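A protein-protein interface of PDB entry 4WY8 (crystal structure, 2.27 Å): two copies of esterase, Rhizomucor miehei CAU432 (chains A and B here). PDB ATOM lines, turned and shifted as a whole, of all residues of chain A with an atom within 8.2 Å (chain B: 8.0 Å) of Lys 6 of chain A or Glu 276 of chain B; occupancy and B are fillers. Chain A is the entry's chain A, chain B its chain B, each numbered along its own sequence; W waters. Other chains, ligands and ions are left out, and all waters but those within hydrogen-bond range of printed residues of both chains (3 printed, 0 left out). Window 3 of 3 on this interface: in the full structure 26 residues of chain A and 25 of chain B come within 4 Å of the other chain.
Of the printed residues of chain B, Thr 4 of chain A touches Arg 272. Of the printed residues of chain B, Lys 8 of chain A touches Ile 275 and Val 281. Of the printed residues of chain B, Glu 259 of chain A touches Arg 272 (2.8 Å). Ala 260 of chain A touches none of the printed residues of chain B. Printed residues of chain B within 4 Å of Leu 287 of chain A: Glu 268 (3.7 Å). Printed residues of chain A within 4 Å of Glu 268 of chain B: Leu 287 (3.7 Å). Of chain A, only Lys 6 comes within 4 Å of Glu 276 of chain B. The nearest residue of chain B that does not touch Lys 6 of chain A is Ile 275 of chain B (4.7 Å).
The backbone carbonyl oxygen of Tyr 286 of chain A is in hydrogen-bond range of the backbone NH of Glu 259 of chain A (3.1 Å). OE1 of Glu 259 of chain A is in hydrogen-bond range of N of Gly 288 of chain A (2.9 Å). O of Gly 288 of chain A lies within hydrogen-bond range of N of Lys 8 of chain A (2.9 Å).
Pro 3 of chain A touches Arg 272 of chain B. Arg 272 of chain B touches Thr 4 of chain A (CD to O, 3.7 Å). Lys 6 of chain A touches Arg 272 of chain B. Lys 6 of chain A touches Glu 276 of chain B. Lys 8 of chain A touches Ile 275 of chain B (CE to CD1, 3.8 Å). Glu 268 of chain B touches Leu 287 of chain A.
Water W2 lies within hydrogen-bond range of the backbone NH of Lys 6 of chain A (2.9 Å), the side-chain carboxylate of Glu 259 of chain A (2.9 Å) and the guanidinium group of Arg 272 of chain B (2.9 Å). Water W3 lies within hydrogen-bond range of the side-chain carboxylate (OE2) of Glu 259 of chain A (3.1 Å) and the side-chain carboxylate (OE1) of Glu 268 of chain B (3.2 Å). Water W1 lies within hydrogen-bond range of the side-chain amino group (NZ) of Lys 8 of chain A (3.5 Å) and the backbone carbonyl oxygen (O) of Val 281 of chain B (3.5 Å).
Of the 18 printed residues of chain A, 6 touch a printed residue of chain B. Hydrophobic or aromatic side chains of chain A within 4 Å of the printed part of chain B: Pro 3 and Leu 287. Of the 18 printed residues of chain B, 5 touch a printed residue of chain A. Printed residues of chain B that touch a printed residue of chain A: Glu 268, Arg 272, Ile 275, Glu 276 and Val 281. Hydrophobic or aromatic side chains of chain B within 4 Å of the printed part of chain A: Ile 275. Among the printed residues, Asp or Glu carboxylates within 4 Å of a Lys or Arg side-chain nitrogen of the other chain: Glu 259 of chain A with Arg 272 of chain B.
The side-chain carboxylate (OE2) of Glu 259 of chain A is in salt-bridge range of the guanidinium group (NH2) of Arg 272 of chain B (2.8 Å). The side-chain amino group (NZ) of Lys 8 of chain A is in hydrogen-bond range of the backbone carbonyl oxygen (O) of Val 281 of chain B (2.7 Å).
No position is printed for both chains. Of the 8 pairs that touch across the chains among the printed residues, none has its exchanged pair printed and touching as well.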
ATOM      1  N   PRO A   3      23.561 -10.997  31.933  1.00  0.00           N
ATOM      2  CA  PRO A   3      22.868 -12.291  32.010  1.00  0.00           C
ATOM      3  C   PRO A   3      23.724 -13.398  32.613  1.00  0.00           C
ATOM      4  O   PRO A   3      24.946 -13.383  32.472  1.00  0.00           O
ATOM      5  CB  PRO A   3      22.526 -12.595  30.542  1.00  0.00           C
ATOM      6  CG  PRO A   3      23.551 -11.850  29.746  1.00  0.00           C
ATOM      7  CD  PRO A   3      23.805 -10.580  30.537  1.00  0.00           C
ATOM      8  N   THR A   4      23.086 -14.344  33.294  1.00  0.00           N
ATOM      9  CA  THR A   4      23.815 -15.471  33.858  1.00  0.00           C
ATOM     10  C   THR A   4      24.009 -16.525  32.765  1.00  0.00           C
ATOM     11  O   THR A   4      23.080 -16.844  32.003  1.00  0.00           O
ATOM     12  CB  THR A   4      23.092 -16.076  35.087  1.00  0.00           C
ATOM     13  OG1 THR A   4      22.475 -17.320  34.739  1.00  0.00           O
ATOM     14  CG2 THR A   4      22.037 -15.114  35.615  1.00  0.00           C
ATOM     15  N   VAL A   5      25.231 -17.047  32.682  1.00  0.00           N
ATOM     16  CA  VAL A   5      25.593 -17.976  31.622  1.00  0.00           C
ATOM     17  C   VAL A   5      24.862 -19.297  31.799  1.00  0.00           C
ATOM     18  O   VAL A   5      24.846 -19.869  32.889  1.00  0.00           O
ATOM     19  CB  VAL A   5      27.124 -18.219  31.592  1.00  0.00           C
ATOM     20  CG1 VAL A   5      27.481 -19.375  30.642  1.00  0.00           C
ATOM     21  CG2 VAL A   5      27.849 -16.932  31.188  1.00  0.00           C
ATOM     22  N   LYS A   6      24.234 -19.772  30.728  1.00  0.00           N
ATOM     23  CA  LYS A   6      23.656 -21.098  30.743  1.00  0.00           C
ATOM     24  C   LYS A   6      24.522 -21.934  29.815  1.00  0.00           C
ATOM     25  O   LYS A   6      24.529 -21.714  28.598  1.00  0.00           O
ATOM     26  CB  LYS A   6      22.189 -21.091  30.288  1.00  0.00           C
ATOM     27  CG  LYS A   6      21.217 -20.272  31.187  1.00  0.00           C
ATOM     28  CD  LYS A   6      21.028 -20.893  32.575  1.00  0.00           C
ATOM     29  CE  LYS A   6      20.015 -20.104  33.415  1.00  0.00           C
ATOM     30  NZ  LYS A   6      20.024 -20.523  34.857  1.00  0.00           N
ATOM     31  N   LEU A   7      25.278 -22.865  30.384  1.00  0.00           N
ATOM     32  CA  LEU A   7      26.098 -23.745  29.574  1.00  0.00           C
ATOM     33  C   LEU A   7      25.245 -24.858  29.007  1.00  0.00           C
ATOM     34  O   LEU A   7      24.240 -25.253  29.609  1.00  0.00           O
ATOM     35  CB  LEU A   7      27.242 -24.354  30.385  1.00  0.00           C
ATOM     36  CG  LEU A   7      28.266 -23.340  30.881  1.00  0.00           C
ATOM     37  CD1 LEU A   7      29.330 -24.067  31.694  1.00  0.00           C
ATOM     38  CD2 LEU A   7      28.857 -22.558  29.716  1.00  0.00           C
ATOM     39  N   LYS A   8      25.650 -25.360  27.845  1.00  0.00           N
ATOM     40  CA  LYS A   8      25.085 -26.588  27.316  1.00  0.00           C
ATOM     41  C   LYS A   8      25.597 -27.770  28.145  1.00  0.00           C
ATOM     42  O   LYS A   8      26.691 -27.710  28.714  1.00  0.00           O
ATOM     43  CB  LYS A   8      25.448 -26.745  25.826  1.00  0.00           C
ATOM     44  CG  LYS A   8      25.090 -25.501  25.016  1.00  0.00           C
ATOM     45  CD  LYS A   8      24.787 -25.813  23.565  1.00  0.00           C
ATOM     46  CE  LYS A   8      24.455 -24.524  22.821  1.00  0.00           C
ATOM     47  NZ  LYS A   8      24.860 -24.538  21.372  1.00  0.00           N
ATOM     48  N   PRO A   9      24.791 -28.842  28.226  1.00  0.00           N
ATOM     49  CA  PRO A   9      25.083 -30.052  29.011  1.00  0.00           C
ATOM     50  C   PRO A   9      26.523 -30.590  28.879  1.00  0.00           C
ATOM     51  O   PRO A   9      27.180 -30.819  29.894  1.00  0.00           O
ATOM     52  CB  PRO A   9      24.064 -31.072  28.465  1.00  0.00           C
ATOM     53  CG  PRO A   9      23.054 -30.245  27.609  1.00  0.00           C
ATOM     54  CD  PRO A   9      23.377 -28.799  27.818  1.00  0.00           C
ATOM     55  N   CYS A  11      29.305 -29.145  27.846  1.00  0.00           N
ATOM     56  CA  CYS A  11      30.262 -28.148  28.323  1.00  0.00           C
ATOM     57  C   CYS A  11      30.181 -27.986  29.839  1.00  0.00           C
ATOM     58  O   CYS A  11      31.199 -27.766  30.506  1.00  0.00           O
ATOM     59  CB  CYS A  11      30.017 -26.801  27.615  1.00  0.00           C
ATOM     60  SG  CYS A  11      30.614 -26.729  25.869  1.00  0.00           S
ATOM     61  N   GLN A  12      28.969 -28.105  30.382  1.00  0.00           N
ATOM     62  CA  GLN A  12      28.794 -28.133  31.831  1.00  0.00           C
ATOM     63  C   GLN A  12      29.569 -29.309  32.422  1.00  0.00           C
ATOM     64  O   GLN A  12      30.408 -29.152  33.333  1.00  0.00           O
ATOM     65  CB  GLN A  12      27.311 -28.246  32.185  1.00  0.00           C
ATOM     66  CG  GLN A  12      27.021 -28.211  33.674  1.00  0.00           C
ATOM     67  CD  GLN A  12      27.278 -26.847  34.289  1.00  0.00           C
ATOM     68  OE1 GLN A  12      26.661 -25.848  33.905  1.00  0.00           O
ATOM     69  NE2 GLN A  12      28.202 -26.798  35.246  1.00  0.00           N
ATOM     70  N   PHE A 207      35.058 -15.422  34.284  1.00  0.00           N
ATOM     71  CA  PHE A 207      35.230 -16.855  34.101  1.00  0.00           C
ATOM     72  C   PHE A 207      36.559 -17.349  34.650  1.00  0.00           C
ATOM     73  O   PHE A 207      37.046 -18.412  34.263  1.00  0.00           O
ATOM     74  CB  PHE A 207      35.095 -17.198  32.622  1.00  0.00           C
ATOM     75  CG  PHE A 207      33.827 -16.663  32.004  1.00  0.00           C
ATOM     76  CD1 PHE A 207      32.597 -17.200  32.350  1.00  0.00           C
ATOM     77  CD2 PHE A 207      33.868 -15.614  31.092  1.00  0.00           C
ATOM     78  CE1 PHE A 207      31.419 -16.708  31.797  1.00  0.00           C
ATOM     79  CE2 PHE A 207      32.700 -15.112  30.515  1.00  0.00           C
ATOM     80  CZ  PHE A 207      31.467 -15.657  30.879  1.00  0.00           C
ATOM     81  N   TYR A 211      35.541 -22.946  34.679  1.00  0.00           N
ATOM     82  CA  TYR A 211      35.158 -23.150  33.277  1.00  0.00           C
ATOM     83  C   TYR A 211      36.283 -23.770  32.438  1.00  0.00           C
ATOM     84  O   TYR A 211      36.516 -23.367  31.271  1.00  0.00           O
ATOM     85  CB  TYR A 211      34.720 -21.830  32.665  1.00  0.00           C
ATOM     86  CG  TYR A 211      33.486 -21.209  33.304  1.00  0.00           C
ATOM     87  CD1 TYR A 211      32.215 -21.550  32.875  1.00  0.00           C
ATOM     88  CD2 TYR A 211      33.607 -20.272  34.338  1.00  0.00           C
ATOM     89  CE1 TYR A 211      31.075 -20.952  33.439  1.00  0.00           C
ATOM     90  CE2 TYR A 211      32.489 -19.685  34.919  1.00  0.00           C
ATOM     91  CZ  TYR A 211      31.224 -20.034  34.465  1.00  0.00           C
ATOM     92  OH  TYR A 211      30.103 -19.458  35.025  1.00  0.00           O
ATOM     93  N   GLU A 259      31.253 -17.942  24.545  1.00  0.00           N
ATOM     94  CA  GLU A 259      30.619 -17.049  25.507  1.00  0.00           C
ATOM     95  C   GLU A 259      31.227 -17.179  26.909  1.00  0.00           C
ATOM     96  O   GLU A 259      31.512 -16.175  27.550  1.00  0.00           O
ATOM     97  CB  GLU A 259      29.120 -17.304  25.575  1.00  0.00           C
ATOM     98  CG  GLU A 259      28.407 -16.371  26.543  1.00  0.00           C
ATOM     99  CD  GLU A 259      26.949 -16.746  26.729  1.00  0.00           C
ATOM    100  OE1 GLU A 259      26.633 -17.949  26.583  1.00  0.00           O
ATOM    101  OE2 GLU A 259      26.131 -15.848  27.052  1.00  0.00           O
ATOM    102  N   ALA A 260      31.416 -18.401  27.396  1.00  0.00           N
ATOM    103  CA  ALA A 260      31.960 -18.566  28.754  1.00  0.00           C
ATOM    104  C   ALA A 260      33.442 -18.919  28.718  1.00  0.00           C
ATOM    105  O   ALA A 260      33.803 -20.068  28.919  1.00  0.00           O
ATOM    106  CB  ALA A 260      31.179 -19.616  29.519  1.00  0.00           C
ATOM    107  N   TYR A 286      29.806 -18.001  19.960  1.00  0.00           N
ATOM    108  CA  TYR A 286      28.849 -19.082  20.186  1.00  0.00           C
ATOM    109  C   TYR A 286      28.378 -19.073  21.622  1.00  0.00           C
ATOM    110  O   TYR A 286      29.199 -19.028  22.551  1.00  0.00           O
ATOM    111  CB  TYR A 286      29.458 -20.435  19.834  1.00  0.00           C
ATOM    112  CG  TYR A 286      29.272 -20.801  18.372  1.00  0.00           C
ATOM    113  CD1 TYR A 286      30.040 -20.196  17.373  1.00  0.00           C
ATOM    114  CD2 TYR A 286      28.346 -21.767  17.992  1.00  0.00           C
ATOM    115  CE1 TYR A 286      29.860 -20.523  16.022  1.00  0.00           C
ATOM    116  CE2 TYR A 286      28.176 -22.113  16.653  1.00  0.00           C
ATOM    117  CZ  TYR A 286      28.938 -21.488  15.681  1.00  0.00           C
ATOM    118  OH  TYR A 286      28.768 -21.840  14.367  1.00  0.00           O
ATOM    119  N   LEU A 287      27.063 -19.127  21.814  1.00  0.00           N
ATOM    120  CA  LEU A 287      26.523 -19.073  23.165  1.00  0.00           C
ATOM    121  C   LEU A 287      26.488 -20.445  23.825  1.00  0.00           C
ATOM    122  O   LEU A 287      26.394 -21.482  23.146  1.00  0.00           O
ATOM    123  CB  LEU A 287      25.129 -18.464  23.169  1.00  0.00           C
ATOM    124  CG  LEU A 287      25.107 -16.950  23.431  1.00  0.00           C
ATOM    125  CD1 LEU A 287      25.632 -16.133  22.239  1.00  0.00           C
ATOM    126  CD2 LEU A 287      23.708 -16.512  23.808  1.00  0.00           C
ATOM    127  N   GLY A 288      26.636 -20.430  25.150  1.00  0.00           N
ATOM    128  CA  GLY A 288      26.534 -21.618  25.974  1.00  0.00           C
ATOM    129  C   GLY A 288      27.705 -22.584  25.937  1.00  0.00           C
ATOM    130  O   GLY A 288      27.582 -23.709  26.424  1.00  0.00           O
ATOM    131  N   ILE A 289      28.850 -22.160  25.403  1.00  0.00           N
ATOM    132  CA  ILE A 289      29.994 -23.061  25.357  1.00  0.00           C
ATOM    133  C   ILE A 289      31.194 -22.524  26.110  1.00  0.00           C
ATOM    134  O   ILE A 289      31.314 -21.325  26.384  1.00  0.00           O
ATOM    135  CB  ILE A 289      30.448 -23.374  23.900  1.00  0.00           C
ATOM    136  CG1 ILE A 289      30.985 -22.121  23.214  1.00  0.00           C
ATOM    137  CG2 ILE A 289      29.325 -23.977  23.094  1.00  0.00           C
ATOM    138  CD1 ILE A 289      31.732 -22.437  21.956  1.00  0.00           C
ATOM    139  N   ILE A 290      32.094 -23.442  26.435  1.00  0.00           N
ATOM    140  CA  ILE A 290      33.333 -23.089  27.083  1.00  0.00           C
ATOM    141  C   ILE A 290      34.510 -23.332  26.172  1.00  0.00           C
ATOM    142  O   ILE A 290      34.401 -23.973  25.126  1.00  0.00           O
ATOM    143  CB  ILE A 290      33.556 -23.884  28.385  1.00  0.00           C
ATOM    144  CG1 ILE A 290      33.505 -25.393  28.091  1.00  0.00           C
ATOM    145  CG2 ILE A 290      32.536 -23.458  29.434  1.00  0.00           C
ATOM    146  CD1 ILE A 290      34.134 -26.281  29.195  1.00  0.00           C
ATOM    147  N   SER B 243       7.432 -20.509  30.094  1.00  0.00           N
ATOM    148  CA  SER B 243       8.150 -21.231  31.124  1.00  0.00           C
ATOM    149  C   SER B 243       9.090 -22.246  30.482  1.00  0.00           C
ATOM    150  O   SER B 243       8.900 -22.614  29.319  1.00  0.00           O
ATOM    151  CB  SER B 243       7.162 -21.933  32.039  1.00  0.00           C
ATOM    152  OG  SER B 243       6.580 -23.031  31.352  1.00  0.00           O
ATOM    153  N   ILE B 244      10.080 -22.727  31.236  1.00  0.00           N
ATOM    154  CA  ILE B 244      10.975 -23.741  30.695  1.00  0.00           C
ATOM    155  C   ILE B 244      10.213 -25.000  30.257  1.00  0.00           C
ATOM    156  O   ILE B 244      10.484 -25.551  29.188  1.00  0.00           O
ATOM    157  CB  ILE B 244      12.067 -24.145  31.699  1.00  0.00           C
ATOM    158  CG1 ILE B 244      12.923 -22.937  32.090  1.00  0.00           C
ATOM    159  CG2 ILE B 244      12.973 -25.192  31.086  1.00  0.00           C
ATOM    160  CD1 ILE B 244      13.511 -22.192  30.915  1.00  0.00           C
ATOM    161  N   ASP B 245       9.235 -25.427  31.045  1.00  0.00           N
ATOM    162  CA  ASP B 245       8.444 -26.617  30.695  1.00  0.00           C
ATOM    163  C   ASP B 245       7.688 -26.403  29.381  1.00  0.00           C
ATOM    164  O   ASP B 245       7.607 -27.305  28.532  1.00  0.00           O
ATOM    165  CB  ASP B 245       7.444 -26.931  31.822  1.00  0.00           C
ATOM    166  CG  ASP B 245       6.763 -28.306  31.672  1.00  0.00           C
ATOM    167  OD1 ASP B 245       7.454 -29.353  31.757  1.00  0.00           O
ATOM    168  OD2 ASP B 245       5.523 -28.325  31.458  1.00  0.00           O
ATOM    169  N   LEU B 247       8.679 -24.860  26.892  1.00  0.00           N
ATOM    170  CA  LEU B 247       9.567 -24.765  25.732  1.00  0.00           C
ATOM    171  C   LEU B 247      10.233 -26.090  25.436  1.00  0.00           C
ATOM    172  O   LEU B 247      11.019 -26.190  24.489  1.00  0.00           O
ATOM    173  CB  LEU B 247      10.639 -23.694  25.956  1.00  0.00           C
ATOM    174  CG  LEU B 247      10.171 -22.236  25.887  1.00  0.00           C
ATOM    175  CD1 LEU B 247      11.299 -21.301  26.305  1.00  0.00           C
ATOM    176  CD2 LEU B 247       9.581 -21.816  24.542  1.00  0.00           C
ATOM    177  N   ARG B 248       9.918 -27.112  26.232  1.00  0.00           N
ATOM    178  CA  ARG B 248      10.477 -28.448  26.028  1.00  0.00           C
ATOM    179  C   ARG B 248      10.045 -29.051  24.698  1.00  0.00           C
ATOM    180  O   ARG B 248       8.969 -28.733  24.188  1.00  0.00           O
ATOM    181  CB  ARG B 248      10.051 -29.376  27.168  1.00  0.00           C
ATOM    182  CG  ARG B 248      10.685 -29.002  28.494  1.00  0.00           C
ATOM    183  CD  ARG B 248      10.660 -30.144  29.499  1.00  0.00           C
ATOM    184  NE  ARG B 248      11.281 -29.731  30.757  1.00  0.00           N
ATOM    185  CZ  ARG B 248      12.562 -29.925  31.051  1.00  0.00           C
ATOM    186  NH1 ARG B 248      13.345 -30.576  30.190  1.00  0.00           N
ATOM    187  NH2 ARG B 248      13.050 -29.497  32.212  1.00  0.00           N
ATOM    188  N   GLU B 268      19.099 -13.588  22.555  1.00  0.00           N
ATOM    189  CA  GLU B 268      19.985 -14.471  23.311  1.00  0.00           C
ATOM    190  C   GLU B 268      19.310 -15.075  24.561  1.00  0.00           C
ATOM    191  O   GLU B 268      19.532 -16.245  24.876  1.00  0.00           O
ATOM    192  CB  GLU B 268      21.265 -13.711  23.658  1.00  0.00           C
ATOM    193  CG  GLU B 268      22.002 -13.339  22.351  1.00  0.00           C
ATOM    194  CD  GLU B 268      23.377 -12.712  22.527  1.00  0.00           C
ATOM    195  OE1 GLU B 268      23.844 -12.518  23.672  1.00  0.00           O
ATOM    196  OE2 GLU B 268      24.010 -12.420  21.483  1.00  0.00           O
ATOM    197  N   ALA B 269      18.452 -14.316  25.245  1.00  0.00           N
ATOM    198  CA  ALA B 269      17.739 -14.875  26.393  1.00  0.00           C
ATOM    199  C   ALA B 269      16.806 -16.013  25.964  1.00  0.00           C
ATOM    200  O   ALA B 269      16.669 -17.025  26.667  1.00  0.00           O
ATOM    201  CB  ALA B 269      16.954 -13.785  27.132  1.00  0.00           C
ATOM    202  N   TYR B 270      16.166 -15.863  24.811  1.00  0.00           N
ATOM    203  CA  TYR B 270      15.281 -16.915  24.340  1.00  0.00           C
ATOM    204  C   TYR B 270      16.096 -18.155  23.999  1.00  0.00           C
ATOM    205  O   TYR B 270      15.697 -19.268  24.341  1.00  0.00           O
ATOM    206  CB  TYR B 270      14.452 -16.447  23.153  1.00  0.00           C
ATOM    207  CG  TYR B 270      13.405 -17.469  22.731  1.00  0.00           C
ATOM    208  CD1 TYR B 270      12.357 -17.804  23.579  1.00  0.00           C
ATOM    209  CD2 TYR B 270      13.465 -18.088  21.485  1.00  0.00           C
ATOM    210  CE1 TYR B 270      11.398 -18.750  23.212  1.00  0.00           C
ATOM    211  CE2 TYR B 270      12.511 -19.023  21.099  1.00  0.00           C
ATOM    212  CZ  TYR B 270      11.476 -19.349  21.970  1.00  0.00           C
ATOM    213  OH  TYR B 270      10.515 -20.273  21.593  1.00  0.00           O
ATOM    214  N   ALA B 271      17.270 -17.974  23.398  1.00  0.00           N
ATOM    215  CA  ALA B 271      18.150 -19.135  23.152  1.00  0.00           C
ATOM    216  C   ALA B 271      18.559 -19.846  24.451  1.00  0.00           C
ATOM    217  O   ALA B 271      18.557 -21.083  24.529  1.00  0.00           O
ATOM    218  CB  ALA B 271      19.393 -18.707  22.388  1.00  0.00           C
ATOM    219  N   ARG B 272      18.929 -19.076  25.470  1.00  0.00           N
ATOM    220  CA  ARG B 272      19.223 -19.682  26.769  1.00  0.00           C
ATOM    221  C   ARG B 272      18.052 -20.490  27.336  1.00  0.00           C
ATOM    222  O   ARG B 272      18.255 -21.598  27.836  1.00  0.00           O
ATOM    223  CB  ARG B 272      19.626 -18.617  27.780  1.00  0.00           C
ATOM    224  CG  ARG B 272      20.989 -18.027  27.518  1.00  0.00           C
ATOM    225  CD  ARG B 272      21.520 -17.222  28.706  1.00  0.00           C
ATOM    226  NE  ARG B 272      22.677 -16.441  28.272  1.00  0.00           N
ATOM    227  CZ  ARG B 272      22.588 -15.206  27.791  1.00  0.00           C
ATOM    228  NH1 ARG B 272      21.408 -14.604  27.728  1.00  0.00           N
ATOM    229  NH2 ARG B 272      23.677 -14.571  27.389  1.00  0.00           N
ATOM    230  N   LYS B 273      16.841 -19.938  27.281  1.00  0.00           N
ATOM    231  CA  LYS B 273      15.671 -20.713  27.711  1.00  0.00           C
ATOM    232  C   LYS B 273      15.514 -21.999  26.903  1.00  0.00           C
ATOM    233  O   LYS B 273      15.231 -23.057  27.461  1.00  0.00           O
ATOM    234  CB  LYS B 273      14.385 -19.887  27.594  1.00  0.00           C
ATOM    235  CG  LYS B 273      14.193 -18.864  28.724  1.00  0.00           C
ATOM    236  CD  LYS B 273      12.712 -18.479  28.895  1.00  0.00           C
ATOM    237  CE  LYS B 273      12.528 -17.456  30.028  1.00  0.00           C
ATOM    238  NZ  LYS B 273      11.075 -17.129  30.271  1.00  0.00           N
ATOM    239  N   LEU B 274      15.696 -21.920  25.591  1.00  0.00           N
ATOM    240  CA  LEU B 274      15.608 -23.133  24.771  1.00  0.00           C
ATOM    241  C   LEU B 274      16.674 -24.158  25.180  1.00  0.00           C
ATOM    242  O   LEU B 274      16.438 -25.361  25.123  1.00  0.00           O
ATOM    243  CB  LEU B 274      15.746 -22.795  23.288  1.00  0.00           C
ATOM    244  CG  LEU B 274      14.627 -21.976  22.636  1.00  0.00           C
ATOM    245  CD1 LEU B 274      15.005 -21.627  21.204  1.00  0.00           C
ATOM    246  CD2 LEU B 274      13.324 -22.762  22.640  1.00  0.00           C
ATOM    247  N   ILE B 275      17.857 -23.689  25.572  1.00  0.00           N
ATOM    248  CA  ILE B 275      18.906 -24.585  26.069  1.00  0.00           C
ATOM    249  C   ILE B 275      18.538 -25.220  27.410  1.00  0.00           C
ATOM    250  O   ILE B 275      18.742 -26.417  27.608  1.00  0.00           O
ATOM    251  CB  ILE B 275      20.244 -23.849  26.187  1.00  0.00           C
ATOM    252  CG1 ILE B 275      20.741 -23.485  24.781  1.00  0.00           C
ATOM    253  CG2 ILE B 275      21.294 -24.701  26.925  1.00  0.00           C
ATOM    254  CD1 ILE B 275      21.908 -22.519  24.789  1.00  0.00           C
ATOM    255  N   GLU B 276      18.015 -24.407  28.323  1.00  0.00           N
ATOM    256  CA  GLU B 276      17.493 -24.864  29.618  1.00  0.00           C
ATOM    257  C   GLU B 276      16.453 -25.973  29.452  1.00  0.00           C
ATOM    258  O   GLU B 276      16.426 -26.939  30.223  1.00  0.00           O
ATOM    259  CB  GLU B 276      16.838 -23.690  30.355  1.00  0.00           C
ATOM    260  CG  GLU B 276      17.778 -22.778  31.162  1.00  0.00           C
ATOM    261  CD  GLU B 276      17.011 -21.726  31.974  1.00  0.00           C
ATOM    262  OE1 GLU B 276      16.971 -20.551  31.537  1.00  0.00           O
ATOM    263  OE2 GLU B 276      16.429 -22.068  33.029  1.00  0.00           O
ATOM    264  N   ALA B 277      15.611 -25.829  28.427  1.00  0.00           N
ATOM    265  CA  ALA B 277      14.524 -26.776  28.160  1.00  0.00           C
ATOM    266  C   ALA B 277      14.988 -28.074  27.485  1.00  0.00           C
ATOM    267  O   ALA B 277      14.155 -28.939  27.159  1.00  0.00           O
ATOM    268  CB  ALA B 277      13.454 -26.096  27.314  1.00  0.00           C
ATOM    269  N   GLY B 278      16.306 -28.215  27.293  1.00  0.00           N
ATOM    270  CA  GLY B 278      16.898 -29.440  26.767  1.00  0.00           C
ATOM    271  C   GLY B 278      16.843 -29.595  25.248  1.00  0.00           C
ATOM    272  O   GLY B 278      17.039 -30.685  24.700  1.00  0.00           O
ATOM    273  N   ASN B 279      16.649 -28.489  24.546  1.00  0.00           N
ATOM    274  CA  ASN B 279      16.575 -28.556  23.096  1.00  0.00           C
ATOM    275  C   ASN B 279      17.948 -28.538  22.417  1.00  0.00           C
ATOM    276  O   ASN B 279      18.974 -28.181  23.031  1.00  0.00           O
ATOM    277  CB  ASN B 279      15.719 -27.402  22.580  1.00  0.00           C
ATOM    278  CG  ASN B 279      14.270 -27.537  22.999  1.00  0.00           C
ATOM    279  OD1 ASN B 279      13.583 -28.485  22.583  1.00  0.00           O
ATOM    280  ND2 ASN B 279      13.795 -26.605  23.831  1.00  0.00           N
ATOM    281  N   VAL B 281      20.001 -26.565  20.360  1.00  0.00           N
ATOM    282  CA  VAL B 281      20.041 -25.136  20.056  1.00  0.00           C
ATOM    283  C   VAL B 281      21.443 -24.640  19.730  1.00  0.00           C
ATOM    284  O   VAL B 281      22.375 -24.853  20.502  1.00  0.00           O
ATOM    285  CB  VAL B 281      19.518 -24.300  21.227  1.00  0.00           C
ATOM    286  CG1 VAL B 281      19.435 -22.832  20.836  1.00  0.00           C
ATOM    287  CG2 VAL B 281      18.143 -24.832  21.663  1.00  0.00           C
HETATM  288  O   HOH W   1      24.612 -27.032  18.973  1.00  0.00           O
HETATM  289  O   HOH W   2      24.264 -18.903  28.010  1.00  0.00           O
HETATM  290  O   HOH W   3      26.552 -13.583  24.954  1.00  0.00           O
